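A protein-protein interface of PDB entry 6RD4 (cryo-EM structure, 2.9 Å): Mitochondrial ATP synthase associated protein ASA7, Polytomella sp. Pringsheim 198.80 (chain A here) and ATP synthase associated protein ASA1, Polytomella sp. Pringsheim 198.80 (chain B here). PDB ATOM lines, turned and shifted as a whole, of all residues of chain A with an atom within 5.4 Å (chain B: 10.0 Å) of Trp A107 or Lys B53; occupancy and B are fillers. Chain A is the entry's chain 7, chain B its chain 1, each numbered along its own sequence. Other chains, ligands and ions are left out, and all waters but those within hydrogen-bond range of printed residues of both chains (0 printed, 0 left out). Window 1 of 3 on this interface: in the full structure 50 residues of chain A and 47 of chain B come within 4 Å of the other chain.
The backbone carbonyl oxygen (O) of Pro B149 is in hydrogen-bond range of the backbone NH (N) of Asp A109 (2.7 Å). The guanidinium group (NE) of Arg B150 lies within hydrogen-bond range of the backbone carbonyl oxygen (O) of Gln A106 (3.0 Å). N of Val B151 lies within hydrogen-bond range of O of Trp A107 (2.9 Å). The backbone carbonyl oxygen (O) of Asp A109 sits close to the side-chain sulfur (SD) of Met B61, at 3.8 Å. The side-chain amino group (NZ) of Lys B53 lies within salt-bridge range of the side-chain carboxylate (OE2) of Glu A136 (3.6 Å).
Hydrophobic or aromatic side chains of chain B within 4 Å of the printed part of chain A: Trp B50, Leu B60, Met B61, Val B151 and Val B153. Printed residues of chain A that touch a printed residue of chain B: Leu A103, Leu A104, Ser A105, Gln A106, Trp A107, Pro A108, Asp A109, Phe A110, Ala A133, Glu A136, Tyr A137 and Leu A140. Hydrophobic or aromatic side chains of chain A that line the printed part of chain B: Leu A103, Leu A104, Trp A107, Pro A108, Ala A133, Tyr A137 and Leu A140. Among the printed residues, 29 pairs touch across the chains. Among the printed residues, Asp or Glu carboxylates within 4 Å of a Lys or Arg side-chain nitrogen of the other chain: Glu A136 with Lys B53.
Trp A107 touches just these residues of chain B: Trp B50, Lys B53, Lys B54, Thr B57, Arg B150 and Val B151. Lys B53 touches two residues of chain A. Of chain B, only Trp B50 comes within 4 Å of Leu A104. Gln A106 touches just these residues of chain B: Lys B54 and Arg B150. Of the printed residues of chain B, Tyr A137 touches Val B151 (3.8 Å) and Val B153 (3.5 Å). Printed residues of chain A within 4 Å of Val B151: Ser A105, Trp A107, Pro A108, Asp A109 and Tyr A137. Printed residues of chain A within 4 Å of Val B153: Ser A105 (3.3 Å) and Tyr A137 (3.5 Å). The nearest residue of chain B that does not touch Trp A107 is Pro B149 (4.4 Å). The nearest printed residue of chain A that does not touch Arg B150 is Phe A110 (6.7 Å).
OE1 of Glu B58 lies close to OE1 of Gln B55 (3.1 Å). O of Phe B148 lies within hydrogen-bond range of NH2 of Arg B150, 3.4 Å away. OH of Tyr A137 is in hydrogen-bond range of O of Leu A104 (3.0 Å). The side-chain hydroxyl (OG1) of Thr B57 is in hydrogen-bond range of the backbone carbonyl oxygen (O) of Lys B53 (2.6 Å). NH1 of Arg B150 lies within salt-bridge range of OE2 of Glu B58 (2.8 Å).
Among the printed residues, merely in contact across the chains: Gln A106 with Lys B54 (3.3 Å), Ser A105 with Val B153 (3.3 Å), Trp A107 with Arg B150 (3.3 Å), Pro A108 with Val B151 (3.5 Å), Pro A108 with Arg B150 (3.5 Å), Tyr A137 with Val B153 (3.5 Å), Pro A108 with Pro B149 (3.5 Å), Trp A107 with Trp B50 (3.5 Å), Leu A103 with Trp B50 (3.6 Å), Trp A107 with Lys B54 (3.6 Å), Trp A107 with Lys B53 (3.6 Å), Pro A108 with Glu B58 (3.6 Å), Asp A109 with Arg B150 (3.6 Å), Phe A110 with Met B61 (3.6 Å), Pro A108 with Met B61 (3.7 Å), Leu A140 with Trp B50 (3.7 Å), Trp A107 with Thr B57 (3.8 Å), Tyr A137 with Val B151 (3.8 Å), Ser A105 with Arg B150 (3.8 Å), Asp A109 with Val B151 (3.8 Å), Ala A133 with Thr B57 (3.9 Å), Ser A105 with Val B151 (3.9 Å), Leu A104 with Trp B50 (3.9 Å) and Ala A133 with Leu B60 (3.9 Å).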
ATOM      1  N   LEU A 103       2.026  31.328 -17.733  1.00  0.00           N
ATOM      2  CA  LEU A 103       3.126  30.401 -17.576  1.00  0.00           C
ATOM      3  C   LEU A 103       3.461  29.654 -18.853  1.00  0.00           C
ATOM      4  O   LEU A 103       4.490  28.982 -18.900  1.00  0.00           O
ATOM      5  CB  LEU A 103       2.848  29.433 -16.430  1.00  0.00           C
ATOM      6  CG  LEU A 103       1.611  28.572 -16.286  1.00  0.00           C
ATOM      7  CD1 LEU A 103       1.845  27.268 -16.903  1.00  0.00           C
ATOM      8  CD2 LEU A 103       1.375  28.364 -14.831  1.00  0.00           C
ATOM      9  N   LEU A 104       2.624  29.740 -19.875  1.00  0.00           N
ATOM     10  CA  LEU A 104       3.055  29.442 -21.226  1.00  0.00           C
ATOM     11  C   LEU A 104       3.743  30.625 -21.875  1.00  0.00           C
ATOM     12  O   LEU A 104       4.304  30.474 -22.956  1.00  0.00           O
ATOM     13  CB  LEU A 104       1.873  29.033 -22.079  1.00  0.00           C
ATOM     14  CG  LEU A 104       1.105  27.817 -21.627  1.00  0.00           C
ATOM     15  CD1 LEU A 104       0.089  27.522 -22.625  1.00  0.00           C
ATOM     16  CD2 LEU A 104       2.006  26.671 -21.531  1.00  0.00           C
ATOM     17  N   SER A 105       3.693  31.797 -21.266  1.00  0.00           N
ATOM     18  CA  SER A 105       4.490  32.915 -21.729  1.00  0.00           C
ATOM     19  C   SER A 105       5.944  32.777 -21.362  1.00  0.00           C
ATOM     20  O   SER A 105       6.786  33.433 -21.972  1.00  0.00           O
ATOM     21  CB  SER A 105       3.979  34.215 -21.135  1.00  0.00           C
ATOM     22  OG  SER A 105       2.705  34.512 -21.630  1.00  0.00           O
ATOM     23  N   GLN A 106       6.246  31.963 -20.363  1.00  0.00           N
ATOM     24  CA  GLN A 106       7.578  31.851 -19.808  1.00  0.00           C
ATOM     25  C   GLN A 106       8.248  30.559 -20.205  1.00  0.00           C
ATOM     26  O   GLN A 106       9.134  30.085 -19.497  1.00  0.00           O
ATOM     27  CB  GLN A 106       7.518  31.972 -18.291  1.00  0.00           C
ATOM     28  CG  GLN A 106       7.095  33.340 -17.832  1.00  0.00           C
ATOM     29  CD  GLN A 106       8.011  34.417 -18.350  1.00  0.00           C
ATOM     30  OE1 GLN A 106       7.568  35.386 -18.960  1.00  0.00           O
ATOM     31  NE2 GLN A 106       9.304  34.253 -18.110  1.00  0.00           N
ATOM     32  N   TRP A 107       7.851  29.992 -21.312  1.00  0.00           N
ATOM     33  CA  TRP A 107       8.334  28.788 -21.947  1.00  0.00           C
ATOM     34  C   TRP A 107       9.533  29.128 -22.810  1.00  0.00           C
ATOM     35  O   TRP A 107       9.492  30.109 -23.550  1.00  0.00           O
ATOM     36  CB  TRP A 107       7.249  28.194 -22.806  1.00  0.00           C
ATOM     37  CG  TRP A 107       7.224  26.746 -22.848  1.00  0.00           C
ATOM     38  CD1 TRP A 107       7.899  25.956 -23.692  1.00  0.00           C
ATOM     39  CD2 TRP A 107       6.449  25.890 -22.024  1.00  0.00           C
ATOM     40  NE1 TRP A 107       7.616  24.649 -23.444  1.00  0.00           N
ATOM     41  CE2 TRP A 107       6.714  24.584 -22.424  1.00  0.00           C
ATOM     42  CE3 TRP A 107       5.558  26.103 -20.979  1.00  0.00           C
ATOM     43  CZ2 TRP A 107       6.135  23.498 -21.822  1.00  0.00           C
ATOM     44  CZ3 TRP A 107       4.978  25.025 -20.388  1.00  0.00           C
ATOM     45  CH2 TRP A 107       5.260  23.741 -20.812  1.00  0.00           C
ATOM     46  N   PRO A 108      10.602  28.340 -22.733  1.00  0.00           N
ATOM     47  CA  PRO A 108      11.815  28.659 -23.480  1.00  0.00           C
ATOM     48  C   PRO A 108      11.615  28.468 -24.967  1.00  0.00           C
ATOM     49  O   PRO A 108      10.894  27.574 -25.406  1.00  0.00           O
ATOM     50  CB  PRO A 108      12.820  27.657 -22.931  1.00  0.00           C
ATOM     51  CG  PRO A 108      11.996  26.542 -22.519  1.00  0.00           C
ATOM     52  CD  PRO A 108      10.762  27.107 -21.963  1.00  0.00           C
ATOM     53  N   ASP A 109      12.249  29.329 -25.752  1.00  0.00           N
ATOM     54  CA  ASP A 109      12.072  29.273 -27.197  1.00  0.00           C
ATOM     55  C   ASP A 109      12.794  28.055 -27.731  1.00  0.00           C
ATOM     56  O   ASP A 109      13.997  28.081 -27.979  1.00  0.00           O
ATOM     57  CB  ASP A 109      12.589  30.528 -27.873  1.00  0.00           C
ATOM     58  CG  ASP A 109      11.860  30.825 -29.148  1.00  0.00           C
ATOM     59  OD1 ASP A 109      11.745  32.006 -29.506  1.00  0.00           O
ATOM     60  OD2 ASP A 109      11.374  29.883 -29.788  1.00  0.00           O
ATOM     61  N   PHE A 110      12.051  26.979 -27.917  1.00  0.00           N
ATOM     62  CA  PHE A 110      12.627  25.766 -28.449  1.00  0.00           C
ATOM     63  C   PHE A 110      12.951  25.875 -29.919  1.00  0.00           C
ATOM     64  O   PHE A 110      13.755  25.096 -30.411  1.00  0.00           O
ATOM     65  CB  PHE A 110      11.686  24.591 -28.216  1.00  0.00           C
ATOM     66  CG  PHE A 110      10.253  24.926 -28.398  1.00  0.00           C
ATOM     67  CD1 PHE A 110       9.456  25.183 -27.319  1.00  0.00           C
ATOM     68  CD2 PHE A 110       9.703  24.978 -29.647  1.00  0.00           C
ATOM     69  CE1 PHE A 110       8.154  25.498 -27.489  1.00  0.00           C
ATOM     70  CE2 PHE A 110       8.397  25.289 -29.813  1.00  0.00           C
ATOM     71  CZ  PHE A 110       7.628  25.550 -28.737  1.00  0.00           C
ATOM     72  N   ALA A 133       8.591  17.571 -27.047  1.00  0.00           N
ATOM     73  CA  ALA A 133       8.321  18.639 -26.101  1.00  0.00           C
ATOM     74  C   ALA A 133       7.961  19.927 -26.810  1.00  0.00           C
ATOM     75  O   ALA A 133       7.434  20.848 -26.189  1.00  0.00           O
ATOM     76  CB  ALA A 133       9.525  18.852 -25.199  1.00  0.00           C
ATOM     77  N   GLU A 136       4.261  19.360 -27.775  1.00  0.00           N
ATOM     78  CA  GLU A 136       3.445  19.401 -26.579  1.00  0.00           C
ATOM     79  C   GLU A 136       3.066  20.820 -26.229  1.00  0.00           C
ATOM     80  O   GLU A 136       1.947  21.061 -25.786  1.00  0.00           O
ATOM     81  CB  GLU A 136       4.217  18.771 -25.441  1.00  0.00           C
ATOM     82  CG  GLU A 136       3.606  18.862 -24.106  1.00  0.00           C
ATOM     83  CD  GLU A 136       4.658  18.696 -23.059  1.00  0.00           C
ATOM     84  OE1 GLU A 136       5.579  19.535 -23.025  1.00  0.00           O
ATOM     85  OE2 GLU A 136       4.599  17.715 -22.301  1.00  0.00           O
ATOM     86  N   TYR A 137       3.979  21.764 -26.439  1.00  0.00           N
ATOM     87  CA  TYR A 137       3.678  23.164 -26.197  1.00  0.00           C
ATOM     88  C   TYR A 137       2.588  23.654 -27.118  1.00  0.00           C
ATOM     89  O   TYR A 137       1.758  24.464 -26.720  1.00  0.00           O
ATOM     90  CB  TYR A 137       4.912  24.015 -26.397  1.00  0.00           C
ATOM     91  CG  TYR A 137       4.661  25.484 -26.246  1.00  0.00           C
ATOM     92  CD1 TYR A 137       4.579  26.047 -24.999  1.00  0.00           C
ATOM     93  CD2 TYR A 137       4.527  26.310 -27.345  1.00  0.00           C
ATOM     94  CE1 TYR A 137       4.365  27.372 -24.852  1.00  0.00           C
ATOM     95  CE2 TYR A 137       4.303  27.624 -27.194  1.00  0.00           C
ATOM     96  CZ  TYR A 137       4.230  28.148 -25.946  1.00  0.00           C
ATOM     97  OH  TYR A 137       4.016  29.474 -25.763  1.00  0.00           O
ATOM     98  N   LEU A 140      -0.597  22.492 -25.576  1.00  0.00           N
ATOM     99  CA  LEU A 140      -1.012  23.260 -24.415  1.00  0.00           C
ATOM    100  C   LEU A 140      -1.429  24.659 -24.807  1.00  0.00           C
ATOM    101  O   LEU A 140      -2.374  25.202 -24.246  1.00  0.00           O
ATOM    102  CB  LEU A 140       0.117  23.343 -23.401  1.00  0.00           C
ATOM    103  CG  LEU A 140       0.761  22.067 -22.917  1.00  0.00           C
ATOM    104  CD1 LEU A 140       1.869  22.397 -21.972  1.00  0.00           C
ATOM    105  CD2 LEU A 140      -0.263  21.217 -22.276  1.00  0.00           C
ATOM    106  N   ASN B  45      -3.496  19.345 -10.150  1.00  0.00           N
ATOM    107  CA  ASN B  45      -2.072  19.464 -10.439  1.00  0.00           C
ATOM    108  C   ASN B  45      -1.922  19.808 -11.911  1.00  0.00           C
ATOM    109  O   ASN B  45      -1.820  18.935 -12.768  1.00  0.00           O
ATOM    110  CB  ASN B  45      -1.345  18.179 -10.083  1.00  0.00           C
ATOM    111  CG  ASN B  45      -0.034  18.440  -9.402  1.00  0.00           C
ATOM    112  OD1 ASN B  45       0.091  19.390  -8.641  1.00  0.00           O
ATOM    113  ND2 ASN B  45       0.951  17.595  -9.663  1.00  0.00           N
ATOM    114  N   LEU B  46      -1.952  21.069 -12.208  1.00  0.00           N
ATOM    115  CA  LEU B  46      -1.674  21.497 -13.564  1.00  0.00           C
ATOM    116  C   LEU B  46      -0.712  22.661 -13.606  1.00  0.00           C
ATOM    117  O   LEU B  46       0.051  22.778 -14.552  1.00  0.00           O
ATOM    118  CB  LEU B  46      -2.963  21.840 -14.285  1.00  0.00           C
ATOM    119  CG  LEU B  46      -2.911  22.219 -15.750  1.00  0.00           C
ATOM    120  CD1 LEU B  46      -3.946  21.458 -16.485  1.00  0.00           C
ATOM    121  CD2 LEU B  46      -3.188  23.676 -15.882  1.00  0.00           C
ATOM    122  N   VAL B  47      -0.718  23.525 -12.601  1.00  0.00           N
ATOM    123  CA  VAL B  47       0.381  24.472 -12.483  1.00  0.00           C
ATOM    124  C   VAL B  47       1.664  23.732 -12.134  1.00  0.00           C
ATOM    125  O   VAL B  47       2.745  24.080 -12.614  1.00  0.00           O
ATOM    126  CB  VAL B  47       0.019  25.570 -11.467  1.00  0.00           C
ATOM    127  CG1 VAL B  47       1.206  26.425 -11.094  1.00  0.00           C
ATOM    128  CG2 VAL B  47      -1.053  26.445 -12.046  1.00  0.00           C
ATOM    129  N   ASN B  48       1.563  22.652 -11.361  1.00  0.00           N
ATOM    130  CA  ASN B  48       2.744  21.850 -11.071  1.00  0.00           C
ATOM    131  C   ASN B  48       3.047  20.805 -12.126  1.00  0.00           C
ATOM    132  O   ASN B  48       4.145  20.261 -12.106  1.00  0.00           O
ATOM    133  CB  ASN B  48       2.619  21.149  -9.726  1.00  0.00           C
ATOM    134  CG  ASN B  48       2.836  22.080  -8.571  1.00  0.00           C
ATOM    135  OD1 ASN B  48       2.007  22.173  -7.674  1.00  0.00           O
ATOM    136  ND2 ASN B  48       3.957  22.786  -8.586  1.00  0.00           N
ATOM    137  N   GLU B  49       2.123  20.488 -13.026  1.00  0.00           N
ATOM    138  CA  GLU B  49       2.501  19.676 -14.173  1.00  0.00           C
ATOM    139  C   GLU B  49       3.006  20.501 -15.331  1.00  0.00           C
ATOM    140  O   GLU B  49       3.865  20.035 -16.075  1.00  0.00           O
ATOM    141  CB  GLU B  49       1.342  18.829 -14.665  1.00  0.00           C
ATOM    142  CG  GLU B  49       1.069  17.659 -13.788  1.00  0.00           C
ATOM    143  CD  GLU B  49      -0.050  16.801 -14.313  1.00  0.00           C
ATOM    144  OE1 GLU B  49      -0.687  17.200 -15.306  1.00  0.00           O
ATOM    145  OE2 GLU B  49      -0.292  15.725 -13.730  1.00  0.00           O
ATOM    146  N   TRP B  50       2.503  21.708 -15.515  1.00  0.00           N
ATOM    147  CA  TRP B  50       3.013  22.530 -16.591  1.00  0.00           C
ATOM    148  C   TRP B  50       4.291  23.230 -16.202  1.00  0.00           C
ATOM    149  O   TRP B  50       4.972  23.766 -17.071  1.00  0.00           O
ATOM    150  CB  TRP B  50       1.990  23.564 -17.025  1.00  0.00           C
ATOM    151  CG  TRP B  50       0.843  23.018 -17.765  1.00  0.00           C
ATOM    152  CD1 TRP B  50       0.491  21.723 -17.886  1.00  0.00           C
ATOM    153  CD2 TRP B  50      -0.114  23.764 -18.497  1.00  0.00           C
ATOM    154  NE1 TRP B  50      -0.631  21.606 -18.645  1.00  0.00           N
ATOM    155  CE2 TRP B  50      -1.024  22.855 -19.033  1.00  0.00           C
ATOM    156  CE3 TRP B  50      -0.292  25.116 -18.749  1.00  0.00           C
ATOM    157  CZ2 TRP B  50      -2.087  23.253 -19.810  1.00  0.00           C
ATOM    158  CZ3 TRP B  50      -1.337  25.505 -19.508  1.00  0.00           C
ATOM    159  CH2 TRP B  50      -2.220  24.584 -20.042  1.00  0.00           C
ATOM    160  N   ASN B  51       4.618  23.277 -14.922  1.00  0.00           N
ATOM    161  CA  ASN B  51       5.941  23.737 -14.548  1.00  0.00           C
ATOM    162  C   ASN B  51       6.970  22.636 -14.667  1.00  0.00           C
ATOM    163  O   ASN B  51       8.156  22.930 -14.796  1.00  0.00           O
ATOM    164  CB  ASN B  51       5.942  24.290 -13.131  1.00  0.00           C
ATOM    165  CG  ASN B  51       5.482  25.711 -13.078  1.00  0.00           C
ATOM    166  OD1 ASN B  51       5.665  26.462 -14.026  1.00  0.00           O
ATOM    167  ND2 ASN B  51       4.877  26.095 -11.975  1.00  0.00           N
ATOM    168  N   ASN B  52       6.537  21.382 -14.613  1.00  0.00           N
ATOM    169  CA  ASN B  52       7.438  20.279 -14.897  1.00  0.00           C
ATOM    170  C   ASN B  52       7.753  20.207 -16.374  1.00  0.00           C
ATOM    171  O   ASN B  52       8.881  19.893 -16.754  1.00  0.00           O
ATOM    172  CB  ASN B  52       6.824  18.973 -14.434  1.00  0.00           C
ATOM    173  CG  ASN B  52       6.777  18.864 -12.953  1.00  0.00           C
ATOM    174  OD1 ASN B  52       7.454  19.599 -12.246  1.00  0.00           O
ATOM    175  ND2 ASN B  52       5.978  17.937 -12.463  1.00  0.00           N
ATOM    176  N   LYS B  53       6.770  20.482 -17.219  1.00  0.00           N
ATOM    177  CA  LYS B  53       7.000  20.456 -18.649  1.00  0.00           C
ATOM    178  C   LYS B  53       7.859  21.615 -19.097  1.00  0.00           C
ATOM    179  O   LYS B  53       8.622  21.474 -20.050  1.00  0.00           O
ATOM    180  CB  LYS B  53       5.676  20.470 -19.380  1.00  0.00           C
ATOM    181  CG  LYS B  53       4.857  19.268 -19.114  1.00  0.00           C
ATOM    182  CD  LYS B  53       3.493  19.418 -19.684  1.00  0.00           C
ATOM    183  CE  LYS B  53       2.741  18.143 -19.532  1.00  0.00           C
ATOM    184  NZ  LYS B  53       1.538  18.157 -20.369  1.00  0.00           N
ATOM    185  N   LYS B  54       7.749  22.763 -18.443  1.00  0.00           N
ATOM    186  CA  LYS B  54       8.654  23.859 -18.747  1.00  0.00           C
ATOM    187  C   LYS B  54      10.054  23.542 -18.270  1.00  0.00           C
ATOM    188  O   LYS B  54      11.030  23.975 -18.882  1.00  0.00           O
ATOM    189  CB  LYS B  54       8.140  25.147 -18.113  1.00  0.00           C
ATOM    190  CG  LYS B  54       8.954  26.373 -18.367  1.00  0.00           C
ATOM    191  CD  LYS B  54       8.616  27.440 -17.380  1.00  0.00           C
ATOM    192  CE  LYS B  54       9.856  28.171 -16.956  1.00  0.00           C
ATOM    193  NZ  LYS B  54       9.556  29.304 -16.049  1.00  0.00           N
ATOM    194  N   GLN B  55      10.176  22.773 -17.195  1.00  0.00           N
ATOM    195  CA  GLN B  55      11.493  22.386 -16.722  1.00  0.00           C
ATOM    196  C   GLN B  55      12.060  21.235 -17.523  1.00  0.00           C
ATOM    197  O   GLN B  55      13.273  21.157 -17.692  1.00  0.00           O
ATOM    198  CB  GLN B  55      11.442  22.029 -15.246  1.00  0.00           C
ATOM    199  CG  GLN B  55      12.769  22.169 -14.561  1.00  0.00           C
ATOM    200  CD  GLN B  55      13.392  23.532 -14.780  1.00  0.00           C
ATOM    201  OE1 GLN B  55      12.739  24.565 -14.627  1.00  0.00           O
ATOM    202  NE2 GLN B  55      14.666  23.541 -15.138  1.00  0.00           N
ATOM    203  N   ALA B  56      11.210  20.341 -18.018  1.00  0.00           N
ATOM    204  CA  ALA B  56      11.676  19.295 -18.914  1.00  0.00           C
ATOM    205  C   ALA B  56      12.160  19.874 -20.229  1.00  0.00           C
ATOM    206  O   ALA B  56      13.156  19.414 -20.782  1.00  0.00           O
ATOM    207  CB  ALA B  56      10.565  18.288 -19.162  1.00  0.00           C
ATOM    208  N   THR B  57      11.478  20.891 -20.735  1.00  0.00           N
ATOM    209  CA  THR B  57      11.912  21.546 -21.957  1.00  0.00           C
ATOM    210  C   THR B  57      13.148  22.399 -21.727  1.00  0.00           C
ATOM    211  O   THR B  57      13.955  22.562 -22.635  1.00  0.00           O
ATOM    212  CB  THR B  57      10.766  22.377 -22.513  1.00  0.00           C
ATOM    213  OG1 THR B  57       9.575  21.597 -22.455  1.00  0.00           O
ATOM    214  CG2 THR B  57      11.005  22.754 -23.935  1.00  0.00           C
ATOM    215  N   GLU B  58      13.323  22.961 -20.538  1.00  0.00           N
ATOM    216  CA  GLU B  58      14.574  23.649 -20.261  1.00  0.00           C
ATOM    217  C   GLU B  58      15.698  22.665 -20.011  1.00  0.00           C
ATOM    218  O   GLU B  58      16.862  22.998 -20.215  1.00  0.00           O
ATOM    219  CB  GLU B  58      14.421  24.587 -19.075  1.00  0.00           C
ATOM    220  CG  GLU B  58      13.770  25.896 -19.430  1.00  0.00           C
ATOM    221  CD  GLU B  58      13.450  26.753 -18.231  1.00  0.00           C
ATOM    222  OE1 GLU B  58      13.572  26.258 -17.095  1.00  0.00           O
ATOM    223  OE2 GLU B  58      13.067  27.924 -18.425  1.00  0.00           O
ATOM    224  N   ASN B  59      15.379  21.461 -19.557  1.00  0.00           N
ATOM    225  CA  ASN B  59      16.406  20.444 -19.423  1.00  0.00           C
ATOM    226  C   ASN B  59      16.818  19.901 -20.773  1.00  0.00           C
ATOM    227  O   ASN B  59      17.996  19.627 -21.001  1.00  0.00           O
ATOM    228  CB  ASN B  59      15.913  19.304 -18.555  1.00  0.00           C
ATOM    229  CG  ASN B  59      15.896  19.653 -17.114  1.00  0.00           C
ATOM    230  OD1 ASN B  59      16.408  20.690 -16.710  1.00  0.00           O
ATOM    231  ND2 ASN B  59      15.301  18.787 -16.312  1.00  0.00           N
ATOM    232  N   LEU B  60      15.860  19.720 -21.675  1.00  0.00           N
ATOM    233  CA  LEU B  60      16.184  19.233 -23.006  1.00  0.00           C
ATOM    234  C   LEU B  60      16.940  20.272 -23.798  1.00  0.00           C
ATOM    235  O   LEU B  60      17.865  19.935 -24.525  1.00  0.00           O
ATOM    236  CB  LEU B  60      14.922  18.843 -23.747  1.00  0.00           C
ATOM    237  CG  LEU B  60      14.345  17.510 -23.341  1.00  0.00           C
ATOM    238  CD1 LEU B  60      12.904  17.456 -23.750  1.00  0.00           C
ATOM    239  CD2 LEU B  60      15.129  16.417 -23.998  1.00  0.00           C
ATOM    240  N   MET B  61      16.566  21.534 -23.673  1.00  0.00           N
ATOM    241  CA  MET B  61      17.278  22.577 -24.387  1.00  0.00           C
ATOM    242  C   MET B  61      18.666  22.795 -23.814  1.00  0.00           C
ATOM    243  O   MET B  61      19.569  23.209 -24.536  1.00  0.00           O
ATOM    244  CB  MET B  61      16.479  23.871 -24.351  1.00  0.00           C
ATOM    245  CG  MET B  61      15.305  23.890 -25.280  1.00  0.00           C
ATOM    246  SD  MET B  61      14.493  25.467 -25.335  1.00  0.00           S
ATOM    247  CE  MET B  61      15.863  26.534 -25.678  1.00  0.00           C
ATOM    248  N   ALA B 147      19.861  30.425 -19.758  1.00  0.00           N
ATOM    249  CA  ALA B 147      19.388  31.763 -20.106  1.00  0.00           C
ATOM    250  C   ALA B 147      18.886  31.704 -21.539  1.00  0.00           C
ATOM    251  O   ALA B 147      19.561  32.144 -22.468  1.00  0.00           O
ATOM    252  CB  ALA B 147      20.473  32.781 -19.943  1.00  0.00           C
ATOM    253  N   PHE B 148      17.689  31.194 -21.711  1.00  0.00           N
ATOM    254  CA  PHE B 148      17.135  31.051 -23.035  1.00  0.00           C
ATOM    255  C   PHE B 148      16.115  32.144 -23.282  1.00  0.00           C
ATOM    256  O   PHE B 148      15.488  32.626 -22.339  1.00  0.00           O
ATOM    257  CB  PHE B 148      16.453  29.690 -23.204  1.00  0.00           C
ATOM    258  CG  PHE B 148      17.380  28.530 -23.093  1.00  0.00           C
ATOM    259  CD1 PHE B 148      18.552  28.496 -23.809  1.00  0.00           C
ATOM    260  CD2 PHE B 148      17.077  27.473 -22.266  1.00  0.00           C
ATOM    261  CE1 PHE B 148      19.401  27.433 -23.706  1.00  0.00           C
ATOM    262  CE2 PHE B 148      17.926  26.409 -22.158  1.00  0.00           C
ATOM    263  CZ  PHE B 148      19.089  26.390 -22.879  1.00  0.00           C
ATOM    264  N   PRO B 149      15.924  32.574 -24.521  1.00  0.00           N
ATOM    265  CA  PRO B 149      14.815  33.477 -24.806  1.00  0.00           C
ATOM    266  C   PRO B 149      13.496  32.741 -24.697  1.00  0.00           C
ATOM    267  O   PRO B 149      13.420  31.521 -24.816  1.00  0.00           O
ATOM    268  CB  PRO B 149      15.084  33.931 -26.240  1.00  0.00           C
ATOM    269  CG  PRO B 149      15.893  32.865 -26.810  1.00  0.00           C
ATOM    270  CD  PRO B 149      16.743  32.334 -25.715  1.00  0.00           C
ATOM    271  N   ARG B 150      12.446  33.502 -24.454  1.00  0.00           N
ATOM    272  CA  ARG B 150      11.123  32.944 -24.253  1.00  0.00           C
ATOM    273  C   ARG B 150      10.337  32.962 -25.549  1.00  0.00           C
ATOM    274  O   ARG B 150      10.656  33.700 -26.479  1.00  0.00           O
ATOM    275  CB  ARG B 150      10.386  33.722 -23.168  1.00  0.00           C
ATOM    276  CG  ARG B 150      10.999  33.566 -21.805  1.00  0.00           C
ATOM    277  CD  ARG B 150      11.103  32.106 -21.521  1.00  0.00           C
ATOM    278  NE  ARG B 150      11.515  31.756 -20.181  1.00  0.00           N
ATOM    279  CZ  ARG B 150      12.558  30.990 -19.917  1.00  0.00           C
ATOM    280  NH1 ARG B 150      12.868  30.695 -18.668  1.00  0.00           N
ATOM    281  NH2 ARG B 150      13.297  30.533 -20.904  1.00  0.00           N
ATOM    282  N   VAL B 151       9.310  32.118 -25.610  1.00  0.00           N
ATOM    283  CA  VAL B 151       8.463  32.078 -26.789  1.00  0.00           C
ATOM    284  C   VAL B 151       7.668  33.367 -26.861  1.00  0.00           C
ATOM    285  O   VAL B 151       7.067  33.791 -25.870  1.00  0.00           O
ATOM    286  CB  VAL B 151       7.533  30.863 -26.750  1.00  0.00           C
ATOM    287  CG1 VAL B 151       6.764  30.788 -28.009  1.00  0.00           C
ATOM    288  CG2 VAL B 151       8.314  29.629 -26.611  1.00  0.00           C
ATOM    289  N   ALA B 152       7.698  34.019 -28.010  1.00  0.00           N
ATOM    290  CA  ALA B 152       6.934  35.240 -28.194  1.00  0.00           C
ATOM    291  C   ALA B 152       5.461  34.900 -28.258  1.00  0.00           C
ATOM    292  O   ALA B 152       4.997  34.289 -29.219  1.00  0.00           O
ATOM    293  CB  ALA B 152       7.368  35.957 -29.463  1.00  0.00           C
ATOM    294  N   VAL B 153       4.731  35.278 -27.224  1.00  0.00           N
ATOM    295  CA  VAL B 153       3.277  35.188 -27.200  1.00  0.00           C
ATOM    296  C   VAL B 153       2.765  36.605 -27.024  1.00  0.00           C
ATOM    297  O   VAL B 153       3.499  37.475 -26.530  1.00  0.00           O
ATOM    298  CB  VAL B 153       2.790  34.244 -26.081  1.00  0.00           C
ATOM    299  CG1 VAL B 153       3.217  32.864 -26.372  1.00  0.00           C
ATOM    300  CG2 VAL B 153       3.387  34.659 -24.824  1.00  0.00           C
